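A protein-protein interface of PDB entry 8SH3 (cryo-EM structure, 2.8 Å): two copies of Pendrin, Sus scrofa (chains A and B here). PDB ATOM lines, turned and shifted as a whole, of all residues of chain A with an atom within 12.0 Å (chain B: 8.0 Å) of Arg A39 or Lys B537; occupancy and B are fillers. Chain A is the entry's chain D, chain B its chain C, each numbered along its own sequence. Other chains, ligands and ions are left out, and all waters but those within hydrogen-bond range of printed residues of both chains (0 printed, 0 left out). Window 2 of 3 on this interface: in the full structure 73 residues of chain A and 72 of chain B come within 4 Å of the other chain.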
ATOM      1  N   GLU A  29      13.592  25.185  -1.453  1.00  0.00           N
ATOM      2  CA  GLU A  29      14.118  24.782  -2.753  1.00  0.00           C
ATOM      3  C   GLU A  29      13.591  23.411  -3.153  1.00  0.00           C
ATOM      4  O   GLU A  29      13.221  23.192  -4.313  1.00  0.00           O
ATOM      5  CB  GLU A  29      15.644  24.791  -2.736  1.00  0.00           C
ATOM      6  CG  GLU A  29      16.270  24.596  -4.104  1.00  0.00           C
ATOM      7  CD  GLU A  29      16.055  25.788  -5.018  1.00  0.00           C
ATOM      8  OE1 GLU A  29      15.837  26.904  -4.502  1.00  0.00           O
ATOM      9  OE2 GLU A  29      16.104  25.608  -6.252  1.00  0.00           O
ATOM     10  N   PHE A  32       9.799  23.786  -4.034  1.00  0.00           N
ATOM     11  CA  PHE A  32       9.657  24.548  -5.270  1.00  0.00           C
ATOM     12  C   PHE A  32      10.063  23.715  -6.478  1.00  0.00           C
ATOM     13  O   PHE A  32       9.399  23.756  -7.520  1.00  0.00           O
ATOM     14  CB  PHE A  32      10.491  25.827  -5.195  1.00  0.00           C
ATOM     15  CG  PHE A  32      10.354  26.713  -6.398  1.00  0.00           C
ATOM     16  CD1 PHE A  32       9.238  27.514  -6.564  1.00  0.00           C
ATOM     17  CD2 PHE A  32      11.344  26.748  -7.363  1.00  0.00           C
ATOM     18  CE1 PHE A  32       9.114  28.330  -7.668  1.00  0.00           C
ATOM     19  CE2 PHE A  32      11.222  27.562  -8.469  1.00  0.00           C
ATOM     20  CZ  PHE A  32      10.105  28.353  -8.621  1.00  0.00           C
ATOM     21  N   GLN A  33      11.151  22.950  -6.359  1.00  0.00           N
ATOM     22  CA  GLN A  33      11.574  22.108  -7.473  1.00  0.00           C
ATOM     23  C   GLN A  33      10.601  20.958  -7.701  1.00  0.00           C
ATOM     24  O   GLN A  33      10.377  20.547  -8.845  1.00  0.00           O
ATOM     25  CB  GLN A  33      12.988  21.583  -7.230  1.00  0.00           C
ATOM     26  CG  GLN A  33      14.079  22.644  -7.320  1.00  0.00           C
ATOM     27  CD  GLN A  33      14.382  23.075  -8.745  1.00  0.00           C
ATOM     28  OE1 GLN A  33      13.493  23.486  -9.490  1.00  0.00           O
ATOM     29  NE2 GLN A  33      15.646  22.973  -9.131  1.00  0.00           N
ATOM     30  N   GLN A  34      10.022  20.416  -6.627  1.00  0.00           N
ATOM     31  CA  GLN A  34       9.018  19.368  -6.786  1.00  0.00           C
ATOM     32  C   GLN A  34       7.788  19.890  -7.517  1.00  0.00           C
ATOM     33  O   GLN A  34       7.243  19.210  -8.393  1.00  0.00           O
ATOM     34  CB  GLN A  34       8.624  18.791  -5.425  1.00  0.00           C
ATOM     35  CG  GLN A  34       9.737  18.054  -4.695  1.00  0.00           C
ATOM     36  CD  GLN A  34      10.227  16.834  -5.448  1.00  0.00           C
ATOM     37  OE1 GLN A  34      11.340  16.820  -5.973  1.00  0.00           O
ATOM     38  NE2 GLN A  34       9.398  15.798  -5.500  1.00  0.00           N
ATOM     39  N   GLN A  35       7.333  21.096  -7.172  1.00  0.00           N
ATOM     40  CA  GLN A  35       6.130  21.628  -7.805  1.00  0.00           C
ATOM     41  C   GLN A  35       6.429  22.259  -9.160  1.00  0.00           C
ATOM     42  O   GLN A  35       5.624  22.143 -10.091  1.00  0.00           O
ATOM     43  CB  GLN A  35       5.452  22.642  -6.885  1.00  0.00           C
ATOM     44  CG  GLN A  35       4.002  22.919  -7.248  1.00  0.00           C
ATOM     45  CD  GLN A  35       3.309  23.823  -6.249  1.00  0.00           C
ATOM     46  OE1 GLN A  35       3.695  23.888  -5.083  1.00  0.00           O
ATOM     47  NE2 GLN A  35       2.280  24.528  -6.703  1.00  0.00           N
ATOM     48  N   TYR A  36       7.573  22.925  -9.295  1.00  0.00           N
ATOM     49  CA  TYR A  36       7.951  23.612 -10.529  1.00  0.00           C
ATOM     50  C   TYR A  36       9.247  22.991 -11.040  1.00  0.00           C
ATOM     51  O   TYR A  36      10.337  23.333 -10.571  1.00  0.00           O
ATOM     52  CB  TYR A  36       8.099  25.112 -10.293  1.00  0.00           C
ATOM     53  CG  TYR A  36       6.824  25.775  -9.824  1.00  0.00           C
ATOM     54  CD1 TYR A  36       5.773  25.999 -10.701  1.00  0.00           C
ATOM     55  CD2 TYR A  36       6.669  26.167  -8.502  1.00  0.00           C
ATOM     56  CE1 TYR A  36       4.605  26.601 -10.276  1.00  0.00           C
ATOM     57  CE2 TYR A  36       5.506  26.770  -8.068  1.00  0.00           C
ATOM     58  CZ  TYR A  36       4.478  26.983  -8.959  1.00  0.00           C
ATOM     59  OH  TYR A  36       3.317  27.585  -8.530  1.00  0.00           O
ATOM     60  N   GLU A  37       9.125  22.081 -12.003  1.00  0.00           N
ATOM     61  CA  GLU A  37      10.288  21.380 -12.528  1.00  0.00           C
ATOM     62  C   GLU A  37      11.144  22.306 -13.383  1.00  0.00           C
ATOM     63  O   GLU A  37      10.631  23.156 -14.114  1.00  0.00           O
ATOM     64  CB  GLU A  37       9.850  20.166 -13.347  1.00  0.00           C
ATOM     65  CG  GLU A  37       9.016  19.160 -12.573  1.00  0.00           C
ATOM     66  CD  GLU A  37       7.527  19.374 -12.755  1.00  0.00           C
ATOM     67  OE1 GLU A  37       7.146  20.264 -13.544  1.00  0.00           O
ATOM     68  OE2 GLU A  37       6.739  18.652 -12.109  1.00  0.00           O
ATOM     69  N   ARG A  38      12.458  22.129 -13.288  1.00  0.00           N
ATOM     70  CA  ARG A  38      13.404  22.902 -14.075  1.00  0.00           C
ATOM     71  C   ARG A  38      13.505  22.273 -15.469  1.00  0.00           C
ATOM     72  O   ARG A  38      12.795  21.315 -15.794  1.00  0.00           O
ATOM     73  CB  ARG A  38      14.746  22.961 -13.340  1.00  0.00           C
ATOM     74  CG  ARG A  38      15.849  23.802 -13.976  1.00  0.00           C
ATOM     75  CD  ARG A  38      17.096  23.830 -13.114  1.00  0.00           C
ATOM     76  NE  ARG A  38      16.900  24.549 -11.863  1.00  0.00           N
ATOM     77  CZ  ARG A  38      17.781  24.570 -10.872  1.00  0.00           C
ATOM     78  NH1 ARG A  38      18.945  23.948 -10.970  1.00  0.00           N
ATOM     79  NH2 ARG A  38      17.487  25.227  -9.755  1.00  0.00           N
ATOM     80  N   ARG A  39      14.377  22.823 -16.314  1.00  0.00           N
ATOM     81  CA  ARG A  39      14.652  22.292 -17.649  1.00  0.00           C
ATOM     82  C   ARG A  39      13.413  22.338 -18.536  1.00  0.00           C
ATOM     83  O   ARG A  39      13.500  22.669 -19.718  1.00  0.00           O
ATOM     84  CB  ARG A  39      15.185  20.858 -17.565  1.00  0.00           C
ATOM     85  CG  ARG A  39      16.553  20.728 -16.918  1.00  0.00           C
ATOM     86  CD  ARG A  39      17.665  21.059 -17.898  1.00  0.00           C
ATOM     87  NE  ARG A  39      18.983  20.922 -17.291  1.00  0.00           N
ATOM     88  CZ  ARG A  39      20.126  21.171 -17.916  1.00  0.00           C
ATOM     89  NH1 ARG A  39      20.150  21.576 -19.175  1.00  0.00           N
ATOM     90  NH2 ARG A  39      21.272  21.009 -17.261  1.00  0.00           N
ATOM     91  N   ASP A 697      19.977  29.453  -8.894  1.00  0.00           N
ATOM     92  CA  ASP A 697      19.922  28.093  -9.419  1.00  0.00           C
ATOM     93  C   ASP A 697      21.317  27.540  -9.681  1.00  0.00           C
ATOM     94  O   ASP A 697      21.614  26.391  -9.332  1.00  0.00           O
ATOM     95  CB  ASP A 697      19.088  28.065 -10.699  1.00  0.00           C
ATOM     96  CG  ASP A 697      17.606  28.225 -10.432  1.00  0.00           C
ATOM     97  OD1 ASP A 697      17.169  27.917  -9.305  1.00  0.00           O
ATOM     98  OD2 ASP A 697      16.878  28.659 -11.350  1.00  0.00           O
ATOM     99  N   HIS A 698      22.190  28.345 -10.292  1.00  0.00           N
ATOM    100  CA  HIS A 698      23.524  27.861 -10.629  1.00  0.00           C
ATOM    101  C   HIS A 698      24.375  27.635  -9.386  1.00  0.00           C
ATOM    102  O   HIS A 698      25.196  26.713  -9.360  1.00  0.00           O
ATOM    103  CB  HIS A 698      24.217  28.835 -11.583  1.00  0.00           C
ATOM    104  CG  HIS A 698      24.476  30.186 -10.993  1.00  0.00           C
ATOM    105  ND1 HIS A 698      23.495  31.146 -10.872  1.00  0.00           N
ATOM    106  CD2 HIS A 698      25.608  30.739 -10.499  1.00  0.00           C
ATOM    107  CE1 HIS A 698      24.012  32.232 -10.325  1.00  0.00           C
ATOM    108  NE2 HIS A 698      25.291  32.011 -10.087  1.00  0.00           N
ATOM    109  N   VAL A 699      24.190  28.449  -8.346  1.00  0.00           N
ATOM    110  CA  VAL A 699      24.955  28.248  -7.120  1.00  0.00           C
ATOM    111  C   VAL A 699      24.518  26.964  -6.424  1.00  0.00           C
ATOM    112  O   VAL A 699      25.344  26.222  -5.881  1.00  0.00           O
ATOM    113  CB  VAL A 699      24.824  29.472  -6.197  1.00  0.00           C
ATOM    114  CG1 VAL A 699      25.602  29.247  -4.916  1.00  0.00           C
ATOM    115  CG2 VAL A 699      25.310  30.722  -6.903  1.00  0.00           C
ATOM    116  N   ILE A 700      23.216  26.674  -6.436  1.00  0.00           N
ATOM    117  CA  ILE A 700      22.732  25.420  -5.865  1.00  0.00           C
ATOM    118  C   ILE A 700      23.212  24.233  -6.697  1.00  0.00           C
ATOM    119  O   ILE A 700      23.520  23.164  -6.157  1.00  0.00           O
ATOM    120  CB  ILE A 700      21.199  25.454  -5.733  1.00  0.00           C
ATOM    121  CG1 ILE A 700      20.791  26.472  -4.668  1.00  0.00           C
ATOM    122  CG2 ILE A 700      20.653  24.084  -5.374  1.00  0.00           C
ATOM    123  CD1 ILE A 700      19.344  26.885  -4.739  1.00  0.00           C
ATOM    124  N   GLU A 701      23.293  24.403  -8.019  1.00  0.00           N
ATOM    125  CA  GLU A 701      23.870  23.357  -8.860  1.00  0.00           C
ATOM    126  C   GLU A 701      25.333  23.115  -8.511  1.00  0.00           C
ATOM    127  O   GLU A 701      25.790  21.966  -8.470  1.00  0.00           O
ATOM    128  CB  GLU A 701      23.731  23.731 -10.335  1.00  0.00           C
ATOM    129  CG  GLU A 701      22.321  23.615 -10.883  1.00  0.00           C
ATOM    130  CD  GLU A 701      22.195  24.193 -12.278  1.00  0.00           C
ATOM    131  OE1 GLU A 701      23.237  24.368 -12.945  1.00  0.00           O
ATOM    132  OE2 GLU A 701      21.057  24.475 -12.708  1.00  0.00           O
ATOM    133  N   LYS A 702      26.087  24.187  -8.267  1.00  0.00           N
ATOM    134  CA  LYS A 702      27.480  24.036  -7.857  1.00  0.00           C
ATOM    135  C   LYS A 702      27.580  23.343  -6.505  1.00  0.00           C
ATOM    136  O   LYS A 702      28.483  22.531  -6.279  1.00  0.00           O
ATOM    137  CB  LYS A 702      28.167  25.399  -7.811  1.00  0.00           C
ATOM    138  CG  LYS A 702      29.657  25.337  -8.082  1.00  0.00           C
ATOM    139  CD  LYS A 702      29.926  24.907  -9.512  1.00  0.00           C
ATOM    140  CE  LYS A 702      31.343  25.233  -9.925  1.00  0.00           C
ATOM    141  NZ  LYS A 702      31.597  24.895 -11.350  1.00  0.00           N
ATOM    142  N   GLU A 704      25.418  21.137  -5.304  1.00  0.00           N
ATOM    143  CA  GLU A 704      25.068  19.728  -5.445  1.00  0.00           C
ATOM    144  C   GLU A 704      26.126  18.955  -6.222  1.00  0.00           C
ATOM    145  O   GLU A 704      26.277  17.746  -6.019  1.00  0.00           O
ATOM    146  CB  GLU A 704      23.696  19.580  -6.107  1.00  0.00           C
ATOM    147  CG  GLU A 704      23.654  19.893  -7.589  1.00  0.00           C
ATOM    148  CD  GLU A 704      22.241  19.939  -8.134  1.00  0.00           C
ATOM    149  OE1 GLU A 704      21.290  19.798  -7.335  1.00  0.00           O
ATOM    150  OE2 GLU A 704      22.079  20.114  -9.359  1.00  0.00           O
ATOM    151  N   GLN A 705      26.869  19.622  -7.107  1.00  0.00           N
ATOM    152  CA  GLN A 705      27.945  18.944  -7.819  1.00  0.00           C
ATOM    153  C   GLN A 705      29.247  18.920  -7.032  1.00  0.00           C
ATOM    154  O   GLN A 705      30.191  18.243  -7.451  1.00  0.00           O
ATOM    155  CB  GLN A 705      28.181  19.596  -9.184  1.00  0.00           C
ATOM    156  CG  GLN A 705      28.850  20.952  -9.126  1.00  0.00           C
ATOM    157  CD  GLN A 705      29.385  21.392 -10.473  1.00  0.00           C
ATOM    158  OE1 GLN A 705      28.701  22.078 -11.232  1.00  0.00           O
ATOM    159  NE2 GLN A 705      30.616  20.999 -10.776  1.00  0.00           N
ATOM    160  N   LYS A 715      18.606  19.381   1.053  1.00  0.00           N
ATOM    161  CA  LYS A 715      18.134  20.562   0.332  1.00  0.00           C
ATOM    162  C   LYS A 715      16.816  21.117   0.867  1.00  0.00           C
ATOM    163  O   LYS A 715      16.211  21.982   0.224  1.00  0.00           O
ATOM    164  CB  LYS A 715      17.995  20.279  -1.171  1.00  0.00           C
ATOM    165  CG  LYS A 715      18.318  21.461  -2.068  1.00  0.00           C
ATOM    166  CD  LYS A 715      17.990  21.152  -3.518  1.00  0.00           C
ATOM    167  CE  LYS A 715      19.105  20.365  -4.182  1.00  0.00           C
ATOM    168  NZ  LYS A 715      18.863  20.188  -5.639  1.00  0.00           N
ATOM    169  N   ILE B 524       6.585  33.261 -11.856  1.00  0.00           N
ATOM    170  CA  ILE B 524       5.706  32.110 -11.638  1.00  0.00           C
ATOM    171  C   ILE B 524       4.278  32.620 -11.501  1.00  0.00           C
ATOM    172  O   ILE B 524       4.047  33.610 -10.778  1.00  0.00           O
ATOM    173  CB  ILE B 524       6.135  31.337 -10.378  1.00  0.00           C
ATOM    174  CG1 ILE B 524       7.559  30.796 -10.519  1.00  0.00           C
ATOM    175  CG2 ILE B 524       5.168  30.204 -10.086  1.00  0.00           C
ATOM    176  CD1 ILE B 524       7.689  29.653 -11.483  1.00  0.00           C
ATOM    177  N   SER B 532      14.362  32.168 -14.283  1.00  0.00           N
ATOM    178  CA  SER B 532      14.751  32.218 -15.686  1.00  0.00           C
ATOM    179  C   SER B 532      13.644  31.658 -16.571  1.00  0.00           C
ATOM    180  O   SER B 532      13.082  30.596 -16.290  1.00  0.00           O
ATOM    181  CB  SER B 532      16.048  31.441 -15.903  1.00  0.00           C
ATOM    182  OG  SER B 532      16.272  31.199 -17.279  1.00  0.00           O
ATOM    183  N   THR B 533      13.330  32.384 -17.646  1.00  0.00           N
ATOM    184  CA  THR B 533      12.220  31.998 -18.511  1.00  0.00           C
ATOM    185  C   THR B 533      12.513  30.719 -19.283  1.00  0.00           C
ATOM    186  O   THR B 533      11.597  29.934 -19.550  1.00  0.00           O
ATOM    187  CB  THR B 533      11.891  33.132 -19.480  1.00  0.00           C
ATOM    188  OG1 THR B 533      13.027  33.395 -20.312  1.00  0.00           O
ATOM    189  CG2 THR B 533      11.535  34.391 -18.718  1.00  0.00           C
ATOM    190  N   LYS B 534      13.770  30.495 -19.652  1.00  0.00           N
ATOM    191  CA  LYS B 534      14.157  29.335 -20.441  1.00  0.00           C
ATOM    192  C   LYS B 534      14.519  28.127 -19.588  1.00  0.00           C
ATOM    193  O   LYS B 534      14.936  27.103 -20.138  1.00  0.00           O
ATOM    194  CB  LYS B 534      15.339  29.690 -21.347  1.00  0.00           C
ATOM    195  CG  LYS B 534      16.636  29.946 -20.600  1.00  0.00           C
ATOM    196  CD  LYS B 534      17.786  30.194 -21.560  1.00  0.00           C
ATOM    197  CE  LYS B 534      19.053  30.572 -20.813  1.00  0.00           C
ATOM    198  NZ  LYS B 534      19.517  29.478 -19.916  1.00  0.00           N
ATOM    199  N   ASP B 535      14.371  28.216 -18.267  1.00  0.00           N
ATOM    200  CA  ASP B 535      14.799  27.155 -17.368  1.00  0.00           C
ATOM    201  C   ASP B 535      13.660  26.355 -16.756  1.00  0.00           C
ATOM    202  O   ASP B 535      13.881  25.207 -16.368  1.00  0.00           O
ATOM    203  CB  ASP B 535      15.652  27.734 -16.232  1.00  0.00           C
ATOM    204  CG  ASP B 535      17.103  27.921 -16.629  1.00  0.00           C
ATOM    205  OD1 ASP B 535      17.387  27.967 -17.843  1.00  0.00           O
ATOM    206  OD2 ASP B 535      17.958  28.027 -15.726  1.00  0.00           O
ATOM    207  N   TYR B 536      12.455  26.918 -16.653  1.00  0.00           N
ATOM    208  CA  TYR B 536      11.389  26.271 -15.901  1.00  0.00           C
ATOM    209  C   TYR B 536      10.187  25.853 -16.736  1.00  0.00           C
ATOM    210  O   TYR B 536       9.373  25.060 -16.252  1.00  0.00           O
ATOM    211  CB  TYR B 536      10.919  27.185 -14.761  1.00  0.00           C
ATOM    212  CG  TYR B 536      11.876  27.188 -13.592  1.00  0.00           C
ATOM    213  CD1 TYR B 536      13.031  27.956 -13.620  1.00  0.00           C
ATOM    214  CD2 TYR B 536      11.639  26.403 -12.474  1.00  0.00           C
ATOM    215  CE1 TYR B 536      13.915  27.953 -12.561  1.00  0.00           C
ATOM    216  CE2 TYR B 536      12.519  26.393 -11.411  1.00  0.00           C
ATOM    217  CZ  TYR B 536      13.654  27.171 -11.461  1.00  0.00           C
ATOM    218  OH  TYR B 536      14.532  27.164 -10.403  1.00  0.00           O
ATOM    219  N   LYS B 537      10.037  26.385 -17.950  1.00  0.00           N
ATOM    220  CA  LYS B 537       9.039  25.934 -18.920  1.00  0.00           C
ATOM    221  C   LYS B 537       7.606  26.234 -18.490  1.00  0.00           C
ATOM    222  O   LYS B 537       6.665  25.993 -19.252  1.00  0.00           O
ATOM    223  CB  LYS B 537       9.192  24.435 -19.200  1.00  0.00           C
ATOM    224  CG  LYS B 537      10.599  23.998 -19.593  1.00  0.00           C
ATOM    225  CD  LYS B 537      11.005  24.523 -20.965  1.00  0.00           C
ATOM    226  CE  LYS B 537      12.000  25.669 -20.853  1.00  0.00           C
ATOM    227  NZ  LYS B 537      12.493  26.112 -22.186  1.00  0.00           N
ATOM    228  N   ASN B 538       7.425  26.756 -17.279  1.00  0.00           N
ATOM    229  CA  ASN B 538       6.135  27.266 -16.833  1.00  0.00           C
ATOM    230  C   ASN B 538       6.202  28.754 -16.526  1.00  0.00           C
ATOM    231  O   ASN B 538       5.236  29.321 -16.006  1.00  0.00           O
ATOM    232  CB  ASN B 538       5.639  26.481 -15.616  1.00  0.00           C
ATOM    233  CG  ASN B 538       6.499  26.698 -14.387  1.00  0.00           C
ATOM    234  OD1 ASN B 538       6.244  27.598 -13.588  1.00  0.00           O
ATOM    235  ND2 ASN B 538       7.532  25.879 -14.239  1.00  0.00           N
ATOM    236  N   ILE B 539       7.323  29.392 -16.841  1.00  0.00           N
ATOM    237  CA  ILE B 539       7.498  30.823 -16.627  1.00  0.00           C
ATOM    238  C   ILE B 539       6.729  31.582 -17.697  1.00  0.00           C
ATOM    239  O   ILE B 539       6.850  31.290 -18.893  1.00  0.00           O
ATOM    240  CB  ILE B 539       8.990  31.190 -16.660  1.00  0.00           C
ATOM    241  CG1 ILE B 539       9.735  30.562 -15.482  1.00  0.00           C
ATOM    242  CG2 ILE B 539       9.153  32.683 -16.651  1.00  0.00           C
ATOM    243  CD1 ILE B 539       9.414  31.192 -14.162  1.00  0.00           C
ATOM    244  N   GLU B 540       5.940  32.565 -17.275  1.00  0.00           N
ATOM    245  CA  GLU B 540       5.181  33.402 -18.193  1.00  0.00           C
ATOM    246  C   GLU B 540       5.897  34.734 -18.389  1.00  0.00           C
ATOM    247  O   GLU B 540       6.278  35.392 -17.416  1.00  0.00           O
ATOM    248  CB  GLU B 540       3.747  33.603 -17.689  1.00  0.00           C
ATOM    249  CG  GLU B 540       3.596  34.283 -16.330  1.00  0.00           C
ATOM    250  CD  GLU B 540       3.569  35.797 -16.419  1.00  0.00           C
ATOM    251  OE1 GLU B 540       3.297  36.326 -17.518  1.00  0.00           O
ATOM    252  OE2 GLU B 540       3.817  36.457 -15.389  1.00  0.00           O
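OD2 of Asp A697 lies within hydrogen-bond range of OH of Tyr B536 (2.9 Å). N of Arg A39 lies within hydrogen-bond range of O of Asp B535, 2.4 Å away. O of Tyr B536 lies close to O of Glu A37 (3.1 Å).
The side-chain hydroxyl (OG) of Ser B532 sits close to the side-chain carboxylate (OD1) of Asp B535, at 3.5 Å. NH1 of Arg A38 lies within salt-bridge range of OE2 of Glu A701, 2.8 Å away. The backbone carbonyl oxygen (O) of Tyr B536 lies within hydrogen-bond range of the side-chain amide nitrogen (ND2) of Asn B538, 2.8 Å away. The guanidinium group (NH2) of Arg A38 sits close to the side-chain amide nitrogen (NE2) of Gln A33, 3.0 Å away. O of Lys B534 is in hydrogen-bond range of NZ of Lys B537 (3.3 Å). The backbone carbonyl oxygen of Tyr A36 sits close to the side-chain amide oxygen of Gln A33 (3.3 Å).
Phe A32 touches Ile B524 (CZ to CD1, 3.96 Å). Tyr B536 touches Phe A32. Gln A33 touches Tyr B536 (OE1 to CE2, 3.6 Å). Tyr A36 touches Ile B524 (CZ to CG2, 3.5 Å). Tyr A36 touches Tyr B536 (O to CD2, 3.8 Å). CD1 of Tyr A36 touches OD1 of Asn B538, 3.3 Å away. Arg A38 touches Asp B535. Arg A38 touches Tyr B536. Lys B537 touches Arg A39 (CG to O, 3.2 Å).
Of the printed residues of chain B, Phe A32 touches Ile B524 and Tyr B536. Printed residues of chain B within 4 Å of Glu A37: Tyr B536 (3.1 Å). Arg A39 touches just these residues of chain B: Asp B535 and Lys B537. Printed residues of chain B within 4 Å of Asp A697: Tyr B536. Glu A701 touches none of the printed residues of chain B. Lys A702 touches none of the printed residues of chain B. Printed residues of chain A within 4 Å of Ile B524: Phe A32 (3.96 Å) and Tyr A36 (3.5 Å). Asp B535 touches just these residues of chain A: Arg A38 (3.1 Å) and Arg A39 (2.4 Å). Printed residues of chain A within 4 Å of Tyr B536: Phe A32, Gln A33, Tyr A36, Glu A37, Arg A38 and Asp A697. Of chain A, only Tyr A36 (3.3 Å) comes within 4 Å of Asn B538.
Among the printed residues, 12 pairs touch across the chains. Among the printed residues, no Asp or Glu carboxylate lies within 4 Å of a Lys or Arg side-chain nitrogen of the other chain.
No position is printed for both chains. Of the 12 pairs that touch across the chains among the printed residues, none has its exchanged pair printed and touching as well.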
